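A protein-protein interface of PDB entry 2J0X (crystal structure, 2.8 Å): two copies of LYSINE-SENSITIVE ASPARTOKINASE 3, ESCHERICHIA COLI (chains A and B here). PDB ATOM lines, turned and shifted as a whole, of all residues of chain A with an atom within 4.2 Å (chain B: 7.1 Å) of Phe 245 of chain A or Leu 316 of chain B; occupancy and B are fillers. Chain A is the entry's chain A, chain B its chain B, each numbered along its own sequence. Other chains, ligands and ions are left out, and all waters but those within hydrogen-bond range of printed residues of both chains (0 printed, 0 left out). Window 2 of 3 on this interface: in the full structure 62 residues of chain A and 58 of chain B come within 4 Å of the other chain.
A ring nitrogen (NE2) of His 260 of chain A sits at hydrogen-bond distance from the backbone carbonyl oxygen of Leu 316 of chain B.
The backbone carbonyl oxygen (O) of Cys 290 of chain A sits at hydrogen-bond distance from the backbone NH (N) of Phe 245 of chain A (2.7 Å). The side-chain hydroxyl (OG) of Ser 315 of chain B sits close to the backbone NH (N) of Asn 317 of chain B, at 3.2 Å.
Leu 316 of chain B touches Phe 245 of chain A. Ala 249 of chain A touches Leu 316 of chain B (CB to CD2, 3.8 Å). Ala 249 of chain A touches Leu 319 of chain B. His 260 of chain A touches Leu 319 of chain B. Pro 261 of chain A touches Leu 319 of chain B. Leu 316 of chain B touches Ala 262 of chain A (CD1 to CA, 3.8 Å). ND2 of Asn 317 of chain B touches CB of Ala 262 of chain A (3.8 Å).
Of the printed residues of chain A, Leu 316 of chain B touches Phe 245, Ala 249, His 260 and Ala 262. Of the printed residues of chain A, Asn 317 of chain B touches Ala 262. Printed residues of chain B within 4 Å of Ala 249 of chain A: Leu 316 and Leu 319. Ile 243 of chain A touches none of the printed residues of chain B. The nearest printed residue of chain B that does not touch Ala 262 of chain A is Leu 319 of chain B (6.1 Å).
Of the 13 printed residues of chain B, 3 touch a printed residue of chain A. Of the 14 printed residues of chain A, 5 touch a printed residue of chain B. Hydrophobic or aromatic side chains of chain A within 4 Å of the printed part of chain B: Phe 245, Ala 249, His 260, Pro 261 and Ala 262. Along chain A the printed residues that touch a printed residue of chain B span positions 245 to 262.
No position is printed for both chains. Of the 8 pairs that touch across the chains among the printed residues, none has its exchanged pair printed and touching as well.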
ATOM      1  N   ILE A 243     -25.549   0.841  -1.596  1.00  0.00           N
ATOM      2  CA  ILE A 243     -24.386   0.489  -0.792  1.00  0.00           C
ATOM      3  C   ILE A 243     -23.570   1.746  -0.566  1.00  0.00           C
ATOM      4  O   ILE A 243     -23.507   2.619  -1.435  1.00  0.00           O
ATOM      5  CB  ILE A 243     -23.475  -0.587  -1.466  1.00  0.00           C
ATOM      6  CG1 ILE A 243     -22.397  -1.025  -0.486  1.00  0.00           C
ATOM      7  CG2 ILE A 243     -22.752  -0.019  -2.675  1.00  0.00           C
ATOM      8  CD1 ILE A 243     -21.775  -2.335  -0.836  1.00  0.00           C
ATOM      9  N   ALA A 244     -22.961   1.844   0.609  1.00  0.00           N
ATOM     10  CA  ALA A 244     -22.138   2.998   0.939  1.00  0.00           C
ATOM     11  C   ALA A 244     -20.788   2.873   0.237  1.00  0.00           C
ATOM     12  O   ALA A 244     -20.279   1.767   0.034  1.00  0.00           O
ATOM     13  CB  ALA A 244     -21.936   3.087   2.440  1.00  0.00           C
ATOM     14  N   PHE A 245     -20.213   4.012  -0.132  1.00  0.00           N
ATOM     15  CA  PHE A 245     -18.932   4.026  -0.815  1.00  0.00           C
ATOM     16  C   PHE A 245     -17.927   3.239  -0.015  1.00  0.00           C
ATOM     17  O   PHE A 245     -17.310   2.301  -0.520  1.00  0.00           O
ATOM     18  CB  PHE A 245     -18.421   5.456  -0.976  1.00  0.00           C
ATOM     19  CG  PHE A 245     -17.133   5.557  -1.752  1.00  0.00           C
ATOM     20  CD1 PHE A 245     -17.050   5.057  -3.052  1.00  0.00           C
ATOM     21  CD2 PHE A 245     -16.016   6.178  -1.199  1.00  0.00           C
ATOM     22  CE1 PHE A 245     -15.874   5.179  -3.793  1.00  0.00           C
ATOM     23  CE2 PHE A 245     -14.830   6.308  -1.930  1.00  0.00           C
ATOM     24  CZ  PHE A 245     -14.759   5.807  -3.233  1.00  0.00           C
ATOM     25  N   ALA A 246     -17.770   3.638   1.242  1.00  0.00           N
ATOM     26  CA  ALA A 246     -16.834   2.998   2.153  1.00  0.00           C
ATOM     27  C   ALA A 246     -16.920   1.469   2.125  1.00  0.00           C
ATOM     28  O   ALA A 246     -15.908   0.775   2.266  1.00  0.00           O
ATOM     29  CB  ALA A 246     -17.062   3.517   3.569  1.00  0.00           C
ATOM     30  N   GLU A 247     -18.127   0.952   1.934  1.00  0.00           N
ATOM     31  CA  GLU A 247     -18.334  -0.485   1.881  1.00  0.00           C
ATOM     32  C   GLU A 247     -17.962  -1.038   0.510  1.00  0.00           C
ATOM     33  O   GLU A 247     -17.244  -2.033   0.397  1.00  0.00           O
ATOM     34  CB  GLU A 247     -19.792  -0.799   2.196  1.00  0.00           C
ATOM     35  CG  GLU A 247     -20.187  -0.452   3.614  1.00  0.00           C
ATOM     36  CD  GLU A 247     -21.658  -0.651   3.856  1.00  0.00           C
ATOM     37  OE1 GLU A 247     -22.459   0.157   3.345  1.00  0.00           O
ATOM     38  OE2 GLU A 247     -22.012  -1.625   4.551  1.00  0.00           O
ATOM     39  N   ALA A 248     -18.458  -0.386  -0.533  1.00  0.00           N
ATOM     40  CA  ALA A 248     -18.178  -0.817  -1.892  1.00  0.00           C
ATOM     41  C   ALA A 248     -16.675  -0.977  -2.092  1.00  0.00           C
ATOM     42  O   ALA A 248     -16.219  -1.962  -2.670  1.00  0.00           O
ATOM     43  CB  ALA A 248     -18.739   0.196  -2.885  1.00  0.00           C
ATOM     44  N   ALA A 249     -15.912  -0.003  -1.606  1.00  0.00           N
ATOM     45  CA  ALA A 249     -14.458  -0.030  -1.729  1.00  0.00           C
ATOM     46  C   ALA A 249     -13.882  -1.303  -1.127  1.00  0.00           C
ATOM     47  O   ALA A 249     -12.959  -1.897  -1.677  1.00  0.00           O
ATOM     48  CB  ALA A 249     -13.852   1.187  -1.044  1.00  0.00           C
ATOM     49  N   HIS A 260     -13.073   0.320 -10.427  1.00  0.00           N
ATOM     50  CA  HIS A 260     -12.212   0.691  -9.306  1.00  0.00           C
ATOM     51  C   HIS A 260     -12.757   1.861  -8.481  1.00  0.00           C
ATOM     52  O   HIS A 260     -12.985   2.948  -9.012  1.00  0.00           O
ATOM     53  CB  HIS A 260     -10.818   1.063  -9.800  1.00  0.00           C
ATOM     54  CG  HIS A 260      -9.835   1.268  -8.691  1.00  0.00           C
ATOM     55  ND1 HIS A 260      -8.894   0.322  -8.347  1.00  0.00           N
ATOM     56  CD2 HIS A 260      -9.713   2.267  -7.785  1.00  0.00           C
ATOM     57  CE1 HIS A 260      -8.237   0.728  -7.274  1.00  0.00           C
ATOM     58  NE2 HIS A 260      -8.716   1.905  -6.913  1.00  0.00           N
ATOM     59  N   PRO A 261     -12.906   1.664  -7.156  1.00  0.00           N
ATOM     60  CA  PRO A 261     -13.419   2.653  -6.202  1.00  0.00           C
ATOM     61  C   PRO A 261     -12.848   4.060  -6.293  1.00  0.00           C
ATOM     62  O   PRO A 261     -13.565   5.041  -6.103  1.00  0.00           O
ATOM     63  CB  PRO A 261     -13.129   2.007  -4.849  1.00  0.00           C
ATOM     64  CG  PRO A 261     -11.913   1.208  -5.120  1.00  0.00           C
ATOM     65  CD  PRO A 261     -12.266   0.555  -6.430  1.00  0.00           C
ATOM     66  N   ALA A 262     -11.558   4.172  -6.573  1.00  0.00           N
ATOM     67  CA  ALA A 262     -10.957   5.493  -6.651  1.00  0.00           C
ATOM     68  C   ALA A 262     -11.615   6.375  -7.711  1.00  0.00           C
ATOM     69  O   ALA A 262     -11.788   7.577  -7.496  1.00  0.00           O
ATOM     70  CB  ALA A 262      -9.461   5.379  -6.911  1.00  0.00           C
ATOM     71  N   VAL A 268     -18.809  10.721  -5.287  1.00  0.00           N
ATOM     72  CA  VAL A 268     -19.156  10.538  -3.883  1.00  0.00           C
ATOM     73  C   VAL A 268     -18.902  11.788  -3.044  1.00  0.00           C
ATOM     74  O   VAL A 268     -19.771  12.208  -2.282  1.00  0.00           O
ATOM     75  CB  VAL A 268     -18.405   9.329  -3.246  1.00  0.00           C
ATOM     76  CG1 VAL A 268     -18.676   8.065  -4.050  1.00  0.00           C
ATOM     77  CG2 VAL A 268     -16.921   9.606  -3.183  1.00  0.00           C
ATOM     78  N   VAL A 289     -24.143   3.455  -5.545  1.00  0.00           N
ATOM     79  CA  VAL A 289     -23.045   3.668  -4.614  1.00  0.00           C
ATOM     80  C   VAL A 289     -23.169   5.102  -4.101  1.00  0.00           C
ATOM     81  O   VAL A 289     -22.941   6.070  -4.823  1.00  0.00           O
ATOM     82  CB  VAL A 289     -21.678   3.446  -5.297  1.00  0.00           C
ATOM     83  CG1 VAL A 289     -20.564   3.492  -4.264  1.00  0.00           C
ATOM     84  CG2 VAL A 289     -21.675   2.110  -6.007  1.00  0.00           C
ATOM     85  N   CYS A 290     -23.555   5.231  -2.844  1.00  0.00           N
ATOM     86  CA  CYS A 290     -23.755   6.539  -2.253  1.00  0.00           C
ATOM     87  C   CYS A 290     -22.717   6.847  -1.198  1.00  0.00           C
ATOM     88  O   CYS A 290     -22.074   5.943  -0.669  1.00  0.00           O
ATOM     89  CB  CYS A 290     -25.148   6.615  -1.624  1.00  0.00           C
ATOM     90  SG  CYS A 290     -26.512   6.218  -2.758  1.00  0.00           S
ATOM     91  N   ASN A 291     -22.572   8.131  -0.890  1.00  0.00           N
ATOM     92  CA  ASN A 291     -21.612   8.572   0.114  1.00  0.00           C
ATOM     93  C   ASN A 291     -21.996   7.937   1.454  1.00  0.00           C
ATOM     94  O   ASN A 291     -21.153   7.368   2.151  1.00  0.00           O
ATOM     95  CB  ASN A 291     -21.626  10.104   0.217  1.00  0.00           C
ATOM     96  CG  ASN A 291     -20.370  10.660   0.874  1.00  0.00           C
ATOM     97  OD1 ASN A 291     -20.178  11.873   0.954  1.00  0.00           O
ATOM     98  ND2 ASN A 291     -19.505   9.769   1.344  1.00  0.00           N
ATOM     99  N   HIS B 314      -4.636   4.234   5.499  1.00  0.00           N
ATOM    100  CA  HIS B 314      -5.741   4.104   4.551  1.00  0.00           C
ATOM    101  C   HIS B 314      -5.489   4.891   3.280  1.00  0.00           C
ATOM    102  O   HIS B 314      -4.990   6.016   3.319  1.00  0.00           O
ATOM    103  CB  HIS B 314      -7.052   4.610   5.145  1.00  0.00           C
ATOM    104  CG  HIS B 314      -8.177   4.673   4.154  1.00  0.00           C
ATOM    105  ND1 HIS B 314      -8.917   3.566   3.791  1.00  0.00           N
ATOM    106  CD2 HIS B 314      -8.663   5.704   3.422  1.00  0.00           C
ATOM    107  CE1 HIS B 314      -9.810   3.914   2.880  1.00  0.00           C
ATOM    108  NE2 HIS B 314      -9.678   5.205   2.639  1.00  0.00           N
ATOM    109  N   SER B 315      -5.848   4.295   2.151  1.00  0.00           N
ATOM    110  CA  SER B 315      -5.697   4.944   0.854  1.00  0.00           C
ATOM    111  C   SER B 315      -6.302   4.132  -0.279  1.00  0.00           C
ATOM    112  O   SER B 315      -5.826   3.043  -0.587  1.00  0.00           O
ATOM    113  CB  SER B 315      -4.234   5.193   0.522  1.00  0.00           C
ATOM    114  OG  SER B 315      -4.136   5.633  -0.826  1.00  0.00           O
ATOM    115  N   LEU B 316      -7.337   4.674  -0.916  1.00  0.00           N
ATOM    116  CA  LEU B 316      -7.991   3.969  -2.013  1.00  0.00           C
ATOM    117  C   LEU B 316      -7.015   3.576  -3.091  1.00  0.00           C
ATOM    118  O   LEU B 316      -7.306   2.708  -3.902  1.00  0.00           O
ATOM    119  CB  LEU B 316      -9.070   4.825  -2.671  1.00  0.00           C
ATOM    120  CG  LEU B 316     -10.432   4.979  -1.995  1.00  0.00           C
ATOM    121  CD1 LEU B 316     -11.320   5.855  -2.877  1.00  0.00           C
ATOM    122  CD2 LEU B 316     -11.063   3.618  -1.785  1.00  0.00           C
ATOM    123  N   ASN B 317      -5.851   4.209  -3.110  1.00  0.00           N
ATOM    124  CA  ASN B 317      -4.894   3.906  -4.160  1.00  0.00           C
ATOM    125  C   ASN B 317      -4.051   2.657  -3.998  1.00  0.00           C
ATOM    126  O   ASN B 317      -3.356   2.275  -4.936  1.00  0.00           O
ATOM    127  CB  ASN B 317      -3.992   5.114  -4.426  1.00  0.00           C
ATOM    128  CG  ASN B 317      -4.698   6.200  -5.223  1.00  0.00           C
ATOM    129  OD1 ASN B 317      -4.143   7.273  -5.460  1.00  0.00           O
ATOM    130  ND2 ASN B 317      -5.928   5.921  -5.646  1.00  0.00           N
ATOM    131  N   MET B 318      -4.094   2.005  -2.842  1.00  0.00           N
ATOM    132  CA  MET B 318      -3.297   0.787  -2.701  1.00  0.00           C
ATOM    133  C   MET B 318      -4.032  -0.353  -3.387  1.00  0.00           C
ATOM    134  O   MET B 318      -3.429  -1.358  -3.739  1.00  0.00           O
ATOM    135  CB  MET B 318      -3.069   0.402  -1.240  1.00  0.00           C
ATOM    136  CG  MET B 318      -4.264  -0.253  -0.575  1.00  0.00           C
ATOM    137  SD  MET B 318      -3.868  -0.710   1.110  1.00  0.00           S
ATOM    138  CE  MET B 318      -3.710   0.929   1.861  1.00  0.00           C
ATOM    139  N   LEU B 319      -5.337  -0.185  -3.576  1.00  0.00           N
ATOM    140  CA  LEU B 319      -6.155  -1.213  -4.207  1.00  0.00           C
ATOM    141  C   LEU B 319      -5.658  -1.525  -5.612  1.00  0.00           C
ATOM    142  O   LEU B 319      -5.744  -0.693  -6.515  1.00  0.00           O
ATOM    143  CB  LEU B 319      -7.620  -0.777  -4.257  1.00  0.00           C
ATOM    144  CG  LEU B 319      -8.669  -1.886  -4.096  1.00  0.00           C
ATOM    145  CD1 LEU B 319     -10.044  -1.270  -4.244  1.00  0.00           C
ATOM    146  CD2 LEU B 319      -8.482  -2.996  -5.124  1.00  0.00           C
ATOM    147  N   HIS B 320      -5.148  -2.746  -5.772  1.00  0.00           N
ATOM    148  CA  HIS B 320      -4.597  -3.260  -7.030  1.00  0.00           C
ATOM    149  C   HIS B 320      -3.302  -2.596  -7.467  1.00  0.00           C
ATOM    150  O   HIS B 320      -2.814  -2.848  -8.566  1.00  0.00           O
ATOM    151  CB  HIS B 320      -5.619  -3.157  -8.147  1.00  0.00           C
ATOM    152  CG  HIS B 320      -6.784  -4.071  -7.967  1.00  0.00           C
ATOM    153  ND1 HIS B 320      -8.081  -3.688  -8.240  1.00  0.00           N
ATOM    154  CD2 HIS B 320      -6.852  -5.354  -7.540  1.00  0.00           C
ATOM    155  CE1 HIS B 320      -8.896  -4.696  -7.986  1.00  0.00           C
ATOM    156  NE2 HIS B 320      -8.175  -5.718  -7.560  1.00  0.00           N
ATOM    157  N   SER B 321      -2.742  -1.755  -6.605  1.00  0.00           N
ATOM    158  CA  SER B 321      -1.498  -1.076  -6.921  1.00  0.00           C
ATOM    159  C   SER B 321      -0.343  -1.993  -6.535  1.00  0.00           C
ATOM    160  O   SER B 321      -0.506  -2.878  -5.698  1.00  0.00           O
ATOM    161  CB  SER B 321      -1.417   0.237  -6.136  1.00  0.00           C
ATOM    162  OG  SER B 321      -0.184   0.908  -6.350  1.00  0.00           O
ATOM    163  N   GLU B 346      -9.165  -4.256   2.378  1.00  0.00           N
ATOM    164  CA  GLU B 346      -8.929  -4.003   0.974  1.00  0.00           C
ATOM    165  C   GLU B 346      -8.251  -2.687   0.665  1.00  0.00           C
ATOM    166  O   GLU B 346      -7.377  -2.643  -0.192  1.00  0.00           O
ATOM    167  CB  GLU B 346     -10.218  -4.144   0.181  1.00  0.00           C
ATOM    168  CG  GLU B 346     -10.663  -5.603   0.052  1.00  0.00           C
ATOM    169  CD  GLU B 346      -9.560  -6.526  -0.473  1.00  0.00           C
ATOM    170  OE1 GLU B 346      -8.536  -6.703   0.226  1.00  0.00           O
ATOM    171  OE2 GLU B 346      -9.713  -7.080  -1.583  1.00  0.00           O
ATOM    172  N   VAL B 347      -8.615  -1.622   1.369  1.00  0.00           N
ATOM    173  CA  VAL B 347      -7.999  -0.329   1.107  1.00  0.00           C
ATOM    174  C   VAL B 347      -7.326   0.329   2.312  1.00  0.00           C
ATOM    175  O   VAL B 347      -7.167   1.547   2.372  1.00  0.00           O
ATOM    176  CB  VAL B 347      -9.030   0.612   0.462  1.00  0.00           C
ATOM    177  CG1 VAL B 347      -9.384   0.075  -0.918  1.00  0.00           C
ATOM    178  CG2 VAL B 347     -10.286   0.699   1.320  1.00  0.00           C
ATOM    179  N   SER B 348      -6.920  -0.484   3.275  1.00  0.00           N
ATOM    180  CA  SER B 348      -6.237   0.052   4.437  1.00  0.00           C
ATOM    181  C   SER B 348      -5.367  -1.039   5.051  1.00  0.00           C
ATOM    182  O   SER B 348      -5.636  -2.231   4.889  1.00  0.00           O
ATOM    183  CB  SER B 348      -7.243   0.608   5.461  1.00  0.00           C
ATOM    184  OG  SER B 348      -7.875  -0.420   6.196  1.00  0.00           O
ATOM    185  N   LEU B 377       0.962   9.684   1.095  1.00  0.00           N
ATOM    186  CA  LEU B 377       0.303   8.705   0.258  1.00  0.00           C
ATOM    187  C   LEU B 377      -0.727   7.860   0.970  1.00  0.00           C
ATOM    188  O   LEU B 377      -0.982   6.727   0.568  1.00  0.00           O
ATOM    189  CB  LEU B 377       1.327   7.813  -0.449  1.00  0.00           C
ATOM    190  CG  LEU B 377       2.344   7.012   0.356  1.00  0.00           C
ATOM    191  CD1 LEU B 377       3.247   6.245  -0.594  1.00  0.00           C
ATOM    192  CD2 LEU B 377       3.174   7.946   1.212  1.00  0.00           C
ATOM    193  N   CYS B 378      -1.325   8.418   2.019  1.00  0.00           N
ATOM    194  CA  CYS B 378      -2.372   7.724   2.759  1.00  0.00           C
ATOM    195  C   CYS B 378      -2.743   8.429   4.055  1.00  0.00           C
ATOM    196  O   CYS B 378      -1.935   9.129   4.665  1.00  0.00           O
ATOM    197  CB  CYS B 378      -1.977   6.269   3.036  1.00  0.00           C
ATOM    198  SG  CYS B 378      -0.532   6.061   4.080  1.00  0.00           S
